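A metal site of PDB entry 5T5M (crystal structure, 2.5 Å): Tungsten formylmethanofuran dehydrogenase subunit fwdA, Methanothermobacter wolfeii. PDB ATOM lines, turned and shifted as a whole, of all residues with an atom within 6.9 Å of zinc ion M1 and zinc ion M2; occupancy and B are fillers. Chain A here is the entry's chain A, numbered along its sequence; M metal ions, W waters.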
ATOM      1  N   HIS A  57     -35.451   9.366 -17.772  1.00  0.00           N
ATOM      2  CA  HIS A  57     -34.459   8.683 -18.623  1.00  0.00           C
ATOM      3  C   HIS A  57     -34.805   8.900 -20.098  1.00  0.00           C
ATOM      4  O   HIS A  57     -35.648   8.195 -20.655  1.00  0.00           O
ATOM      5  CB  HIS A  57     -34.414   7.200 -18.298  1.00  0.00           C
ATOM      6  CG  HIS A  57     -33.229   6.505 -18.868  1.00  0.00           C
ATOM      7  ND1 HIS A  57     -32.106   6.222 -18.113  1.00  0.00           N
ATOM      8  CD2 HIS A  57     -32.974   6.033 -20.108  1.00  0.00           C
ATOM      9  CE1 HIS A  57     -31.217   5.600 -18.871  1.00  0.00           C
ATOM     10  NE2 HIS A  57     -31.714   5.478 -20.086  1.00  0.00           N
ATOM     11  N   SER A  58     -34.111   9.841 -20.724  1.00  0.00           N
ATOM     12  CA  SER A  58     -34.305  10.159 -22.128  1.00  0.00           C
ATOM     13  C   SER A  58     -32.972  10.567 -22.737  1.00  0.00           C
ATOM     14  O   SER A  58     -32.088  11.058 -22.037  1.00  0.00           O
ATOM     15  CB  SER A  58     -35.346  11.266 -22.280  1.00  0.00           C
ATOM     16  OG  SER A  58     -35.793  11.395 -23.614  1.00  0.00           O
ATOM     17  N   HIS A  59     -32.817  10.343 -24.033  1.00  0.00           N
ATOM     18  CA  HIS A  59     -31.597  10.737 -24.731  1.00  0.00           C
ATOM     19  C   HIS A  59     -31.937  11.917 -25.632  1.00  0.00           C
ATOM     20  O   HIS A  59     -32.403  11.750 -26.755  1.00  0.00           O
ATOM     21  CB  HIS A  59     -31.020   9.558 -25.502  1.00  0.00           C
ATOM     22  CG  HIS A  59     -30.530   8.453 -24.622  1.00  0.00           C
ATOM     23  ND1 HIS A  59     -29.249   8.411 -24.108  1.00  0.00           N
ATOM     24  CD2 HIS A  59     -31.171   7.369 -24.122  1.00  0.00           C
ATOM     25  CE1 HIS A  59     -29.114   7.341 -23.349  1.00  0.00           C
ATOM     26  NE2 HIS A  59     -30.265   6.688 -23.343  1.00  0.00           N
ATOM     27  N   ALA A 115     -29.781  11.181 -20.073  1.00  0.00           N
ATOM     28  CA  ALA A 115     -29.455   9.966 -19.344  1.00  0.00           C
ATOM     29  C   ALA A 115     -27.989   9.535 -19.422  1.00  0.00           C
ATOM     30  O   ALA A 115     -27.570   8.724 -18.600  1.00  0.00           O
ATOM     31  CB  ALA A 115     -30.334   8.822 -19.849  1.00  0.00           C
ATOM     32  N   ALA A 116     -27.198  10.039 -20.395  1.00  0.00           N
ATOM     33  CA  ALA A 116     -25.830   9.536 -20.560  1.00  0.00           C
ATOM     34  C   ALA A 116     -24.937  10.616 -21.155  1.00  0.00           C
ATOM     35  O   ALA A 116     -24.860  10.761 -22.376  1.00  0.00           O
ATOM     36  CB  ALA A 116     -25.839   8.289 -21.428  1.00  0.00           C
ATOM     37  N   KCX A 178     -24.367   7.735 -13.341  1.00  0.00           N
ATOM     38  CA  KCX A 178     -24.893   6.777 -14.346  1.00  0.00           C
ATOM     39  CB  KCX A 178     -25.252   7.542 -15.627  1.00  0.00           C
ATOM     40  CG  KCX A 178     -25.687   6.569 -16.713  1.00  0.00           C
ATOM     41  CD  KCX A 178     -27.071   6.058 -16.341  1.00  0.00           C
ATOM     42  CE  KCX A 178     -27.626   5.085 -17.364  1.00  0.00           C
ATOM     43  NZ  KCX A 178     -27.924   5.738 -18.619  1.00  0.00           N
ATOM     44  C   KCX A 178     -23.876   5.696 -14.659  1.00  0.00           C
ATOM     45  O   KCX A 178     -22.673   6.003 -14.860  1.00  0.00           O
ATOM     46  CX  KCX A 178     -28.219   4.988 -19.669  1.00  0.00           C
ATOM     47  OQ1 KCX A 178     -28.202   3.767 -19.606  1.00  0.00           O
ATOM     48  OQ2 KCX A 178     -28.573   5.561 -20.824  1.00  0.00           O
ATOM     49  N   ILE A 179     -24.318   4.440 -14.670  1.00  0.00           N
ATOM     50  CA  ILE A 179     -23.442   3.292 -14.890  1.00  0.00           C
ATOM     51  C   ILE A 179     -23.962   2.482 -16.077  1.00  0.00           C
ATOM     52  O   ILE A 179     -25.042   1.901 -15.996  1.00  0.00           O
ATOM     53  CB  ILE A 179     -23.365   2.399 -13.627  1.00  0.00           C
ATOM     54  CG1 ILE A 179     -23.130   3.252 -12.378  1.00  0.00           C
ATOM     55  CG2 ILE A 179     -22.281   1.355 -13.786  1.00  0.00           C
ATOM     56  CD1 ILE A 179     -23.168   2.470 -11.078  1.00  0.00           C
ATOM     57  N   VAL A 180     -23.200   2.431 -17.172  1.00  0.00           N
ATOM     58  CA  VAL A 180     -23.618   1.747 -18.389  1.00  0.00           C
ATOM     59  C   VAL A 180     -22.606   0.647 -18.694  1.00  0.00           C
ATOM     60  O   VAL A 180     -21.438   0.934 -18.976  1.00  0.00           O
ATOM     61  CB  VAL A 180     -23.742   2.718 -19.573  1.00  0.00           C
ATOM     62  CG1 VAL A 180     -23.966   1.954 -20.876  1.00  0.00           C
ATOM     63  CG2 VAL A 180     -24.879   3.686 -19.327  1.00  0.00           C
ATOM     64  N   HIS A 229     -27.726   4.931 -11.152  1.00  0.00           N
ATOM     65  CA  HIS A 229     -28.639   4.709 -12.270  1.00  0.00           C
ATOM     66  C   HIS A 229     -27.977   3.625 -13.123  1.00  0.00           C
ATOM     67  O   HIS A 229     -26.998   3.907 -13.824  1.00  0.00           O
ATOM     68  CB  HIS A 229     -28.810   6.019 -13.028  1.00  0.00           C
ATOM     69  CG  HIS A 229     -30.078   6.133 -13.811  1.00  0.00           C
ATOM     70  ND1 HIS A 229     -31.132   6.902 -13.386  1.00  0.00           N
ATOM     71  CD2 HIS A 229     -30.439   5.627 -15.017  1.00  0.00           C
ATOM     72  CE1 HIS A 229     -32.097   6.848 -14.286  1.00  0.00           C
ATOM     73  NE2 HIS A 229     -31.707   6.083 -15.279  1.00  0.00           N
ATOM     74  N   LEU A 230     -28.486   2.397 -13.064  1.00  0.00           N
ATOM     75  CA  LEU A 230     -27.764   1.245 -13.584  1.00  0.00           C
ATOM     76  C   LEU A 230     -28.383   0.701 -14.866  1.00  0.00           C
ATOM     77  O   LEU A 230     -29.577   0.371 -14.904  1.00  0.00           O
ATOM     78  CB  LEU A 230     -27.673   0.127 -12.541  1.00  0.00           C
ATOM     79  CG  LEU A 230     -26.916  -1.121 -13.020  1.00  0.00           C
ATOM     80  CD1 LEU A 230     -25.511  -0.760 -13.484  1.00  0.00           C
ATOM     81  CD2 LEU A 230     -26.855  -2.171 -11.911  1.00  0.00           C
ATOM     82  N   HIS A 231     -27.542   0.599 -15.905  1.00  0.00           N
ATOM     83  CA  HIS A 231     -27.813  -0.085 -17.173  1.00  0.00           C
ATOM     84  C   HIS A 231     -26.923  -1.334 -17.157  1.00  0.00           C
ATOM     85  O   HIS A 231     -25.704  -1.235 -17.286  1.00  0.00           O
ATOM     86  CB  HIS A 231     -27.515   0.883 -18.324  1.00  0.00           C
ATOM     87  CG  HIS A 231     -27.238   0.278 -19.672  1.00  0.00           C
ATOM     88  ND1 HIS A 231     -27.671   0.870 -20.839  1.00  0.00           N
ATOM     89  CD2 HIS A 231     -26.498  -0.804 -20.055  1.00  0.00           C
ATOM     90  CE1 HIS A 231     -27.244   0.176 -21.879  1.00  0.00           C
ATOM     91  NE2 HIS A 231     -26.535  -0.848 -21.431  1.00  0.00           N
ATOM     92  N   CYS A 232     -27.537  -2.505 -16.970  1.00  0.00           N
ATOM     93  CA  CYS A 232     -26.798  -3.713 -16.606  1.00  0.00           C
ATOM     94  C   CYS A 232     -25.919  -4.224 -17.748  1.00  0.00           C
ATOM     95  O   CYS A 232     -26.122  -3.913 -18.916  1.00  0.00           O
ATOM     96  CB  CYS A 232     -27.750  -4.834 -16.187  1.00  0.00           C
ATOM     97  SG  CYS A 232     -28.604  -4.567 -14.643  1.00  0.00           S
ATOM     98  N   LEU A 235     -26.788  -6.512 -21.910  1.00  0.00           N
ATOM     99  CA  LEU A 235     -28.058  -6.015 -22.440  1.00  0.00           C
ATOM    100  C   LEU A 235     -28.455  -6.747 -23.726  1.00  0.00           C
ATOM    101  O   LEU A 235     -27.637  -6.967 -24.632  1.00  0.00           O
ATOM    102  CB  LEU A 235     -27.958  -4.511 -22.712  1.00  0.00           C
ATOM    103  CG  LEU A 235     -29.265  -3.823 -23.157  1.00  0.00           C
ATOM    104  CD1 LEU A 235     -29.289  -2.402 -22.675  1.00  0.00           C
ATOM    105  CD2 LEU A 235     -29.454  -3.848 -24.674  1.00  0.00           C
ATOM    106  N   THR A 270     -32.494   0.911 -15.027  1.00  0.00           N
ATOM    107  CA  THR A 270     -33.183   1.519 -16.155  1.00  0.00           C
ATOM    108  C   THR A 270     -33.423   0.508 -17.285  1.00  0.00           C
ATOM    109  O   THR A 270     -32.722  -0.511 -17.409  1.00  0.00           O
ATOM    110  CB  THR A 270     -32.395   2.719 -16.686  1.00  0.00           C
ATOM    111  OG1 THR A 270     -33.115   3.335 -17.752  1.00  0.00           O
ATOM    112  CG2 THR A 270     -31.008   2.297 -17.170  1.00  0.00           C
ATOM    113  N   HIS A 271     -34.419   0.829 -18.106  1.00  0.00           N
ATOM    114  CA  HIS A 271     -34.917  -0.006 -19.204  1.00  0.00           C
ATOM    115  C   HIS A 271     -34.720  -1.498 -18.961  1.00  0.00           C
ATOM    116  O   HIS A 271     -34.019  -2.177 -19.702  1.00  0.00           O
ATOM    117  CB  HIS A 271     -34.282   0.407 -20.547  1.00  0.00           C
ATOM    118  CG  HIS A 271     -32.789   0.545 -20.528  1.00  0.00           C
ATOM    119  ND1 HIS A 271     -31.939  -0.529 -20.455  1.00  0.00           N
ATOM    120  CD2 HIS A 271     -31.997   1.640 -20.652  1.00  0.00           C
ATOM    121  CE1 HIS A 271     -30.686  -0.103 -20.490  1.00  0.00           C
ATOM    122  NE2 HIS A 271     -30.702   1.210 -20.617  1.00  0.00           N
ATOM    123  N   HIS A 275     -33.398  -6.382 -20.195  1.00  0.00           N
ATOM    124  CA  HIS A 275     -32.606  -7.165 -19.245  1.00  0.00           C
ATOM    125  C   HIS A 275     -33.407  -8.324 -18.645  1.00  0.00           C
ATOM    126  O   HIS A 275     -32.982  -8.902 -17.634  1.00  0.00           O
ATOM    127  CB  HIS A 275     -32.080  -6.241 -18.152  1.00  0.00           C
ATOM    128  CG  HIS A 275     -31.242  -5.120 -18.665  1.00  0.00           C
ATOM    129  ND1 HIS A 275     -29.893  -5.259 -18.895  1.00  0.00           N
ATOM    130  CD2 HIS A 275     -31.543  -3.839 -18.993  1.00  0.00           C
ATOM    131  CE1 HIS A 275     -29.399  -4.114 -19.341  1.00  0.00           C
ATOM    132  NE2 HIS A 275     -30.385  -3.233 -19.395  1.00  0.00           N
ATOM    133  N   MET A 317     -29.301   4.575 -29.425  1.00  0.00           N
ATOM    134  CA  MET A 317     -28.147   5.390 -29.075  1.00  0.00           C
ATOM    135  C   MET A 317     -27.866   5.177 -27.591  1.00  0.00           C
ATOM    136  O   MET A 317     -28.676   5.526 -26.729  1.00  0.00           O
ATOM    137  CB  MET A 317     -28.389   6.866 -29.386  1.00  0.00           C
ATOM    138  CG  MET A 317     -29.742   7.415 -28.933  1.00  0.00           C
ATOM    139  SD  MET A 317     -29.972   9.158 -29.322  1.00  0.00           S
ATOM    140  CE  MET A 317     -29.737   9.176 -31.087  1.00  0.00           C
ATOM    141  N   THR A 318     -26.717   4.575 -27.285  1.00  0.00           N
ATOM    142  CA  THR A 318     -26.385   4.247 -25.913  1.00  0.00           C
ATOM    143  C   THR A 318     -24.888   4.424 -25.710  1.00  0.00           C
ATOM    144  O   THR A 318     -24.116   4.480 -26.666  1.00  0.00           O
ATOM    145  CB  THR A 318     -26.775   2.793 -25.548  1.00  0.00           C
ATOM    146  OG1 THR A 318     -25.897   1.874 -26.206  1.00  0.00           O
ATOM    147  CG2 THR A 318     -28.205   2.507 -25.949  1.00  0.00           C
ATOM    148  N   ALA A 319     -24.501   4.513 -24.446  1.00  0.00           N
ATOM    149  CA  ALA A 319     -23.108   4.450 -24.064  1.00  0.00           C
ATOM    150  C   ALA A 319     -22.600   3.023 -24.003  1.00  0.00           C
ATOM    151  O   ALA A 319     -21.524   2.773 -23.453  1.00  0.00           O
ATOM    152  CB  ALA A 319     -22.913   5.153 -22.710  1.00  0.00           C
ATOM    153  N   ASP A 320     -23.367   2.077 -24.554  1.00  0.00           N
ATOM    154  CA  ASP A 320     -23.012   0.667 -24.590  1.00  0.00           C
ATOM    155  C   ASP A 320     -22.423   0.341 -25.969  1.00  0.00           C
ATOM    156  O   ASP A 320     -23.030  -0.315 -26.821  1.00  0.00           O
ATOM    157  CB  ASP A 320     -24.240  -0.189 -24.260  1.00  0.00           C
ATOM    158  CG  ASP A 320     -23.894  -1.628 -23.931  1.00  0.00           C
ATOM    159  OD1 ASP A 320     -22.801  -2.092 -24.312  1.00  0.00           O
ATOM    160  OD2 ASP A 320     -24.744  -2.297 -23.282  1.00  0.00           O
ATOM    161  N   ASP A 385     -36.595   4.318 -22.969  1.00  0.00           N
ATOM    162  CA  ASP A 385     -35.183   4.614 -23.171  1.00  0.00           C
ATOM    163  C   ASP A 385     -35.036   5.511 -24.391  1.00  0.00           C
ATOM    164  O   ASP A 385     -34.134   5.332 -25.206  1.00  0.00           O
ATOM    165  CB  ASP A 385     -34.364   3.328 -23.339  1.00  0.00           C
ATOM    166  CG  ASP A 385     -32.851   3.575 -23.307  1.00  0.00           C
ATOM    167  OD1 ASP A 385     -32.419   4.600 -22.733  1.00  0.00           O
ATOM    168  OD2 ASP A 385     -32.087   2.733 -23.841  1.00  0.00           O
ATOM    169  N   SER A 386     -35.937   6.487 -24.505  1.00  0.00           N
ATOM    170  CA  SER A 386     -36.091   7.279 -25.709  1.00  0.00           C
ATOM    171  C   SER A 386     -34.753   7.665 -26.346  1.00  0.00           C
ATOM    172  O   SER A 386     -33.889   8.224 -25.683  1.00  0.00           O
ATOM    173  CB  SER A 386     -36.880   8.562 -25.407  1.00  0.00           C
ATOM    174  OG  SER A 386     -37.180   9.270 -26.601  1.00  0.00           O
ATOM    175  N   ASN A 388     -34.425   4.608 -27.890  1.00  0.00           N
ATOM    176  CA  ASN A 388     -33.941   3.244 -28.117  1.00  0.00           C
ATOM    177  C   ASN A 388     -35.088   2.254 -28.336  1.00  0.00           C
ATOM    178  O   ASN A 388     -35.047   1.432 -29.258  1.00  0.00           O
ATOM    179  CB  ASN A 388     -33.071   2.814 -26.942  1.00  0.00           C
ATOM    180  CG  ASN A 388     -31.710   3.486 -26.949  1.00  0.00           C
ATOM    181  OD1 ASN A 388     -30.805   3.056 -27.663  1.00  0.00           O
ATOM    182  ND2 ASN A 388     -31.566   4.544 -26.166  1.00  0.00           N
HETATM  183 ZN    ZN M   1     -30.540   5.189 -21.942  1.00  0.00          ZN
HETATM  184 ZN    ZN M   2     -29.037   2.514 -21.073  1.00  0.00          ZN
HETATM  185  O   HOH W   1     -30.022   3.390 -22.484  1.00  0.00           O
HETATM  186  O   HOH W   2     -26.757   4.412 -22.824  1.00  0.00           O
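N of His 59 is in hydrogen-bond range of O of Ser 386 (2.9 Å).
NZ of KCX 178 sits at hydrogen-bond distance from O of Ala 115, 3.0 Å away.
The backbone carbonyl oxygen (O) of Asp 385 lies within hydrogen-bond range of the side-chain amide nitrogen (ND2) of Asn 388 (2.9 Å).
A ring nitrogen (NE2) of His 231 is in hydrogen-bond range of the side-chain carboxylate (OD2) of Asp 320 (3.0 Å).
The backbone NH (N) of His 231 is in hydrogen-bond range of the backbone carbonyl oxygen (O) of Ile 179 (2.8 Å).
NE2 of His 275 lies within hydrogen-bond range of ND1 of His 271 (3.3 Å).
A ring nitrogen (ND1) of His 57 lies within hydrogen-bond range of the side-chain hydroxyl (OG1) of Thr 270, at 3.1 Å.
A ring nitrogen (ND1) of His 57 sits at hydrogen-bond distance from a ring nitrogen (NE2) of His 229, at 2.9 Å.
Of the 23 residues printed, 4 come within 4 Å of zinc ion M1.
Of the 23 residues printed, 3 come within 4 Å of zinc ion M2.
Zinc ion M1 is bound by water W1 (1.9 Å).
NE2 of His 59 is bound to zinc ion M1.
Zinc ion M1 is bound by OD1 of Asp 385.
Zinc ion M1 is bound by NE2 of His 57.
OQ2 of KCX 178 is bound to zinc ion M1 (2.3 Å).
Zinc ion M1 has five donor atoms within binding distance.
Zinc ion M2 is bound by water W1.
Zinc ion M2 is bound by OQ1 of KCX 178 (2.1 Å).
A ring nitrogen (ND1) of His 231 binds zinc ion M2 (2.2 Å).
Zinc ion M2 is bound by NE2 of His 271, at 2.2 Å.
Zinc ion M2 has four donor atoms within binding distance.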
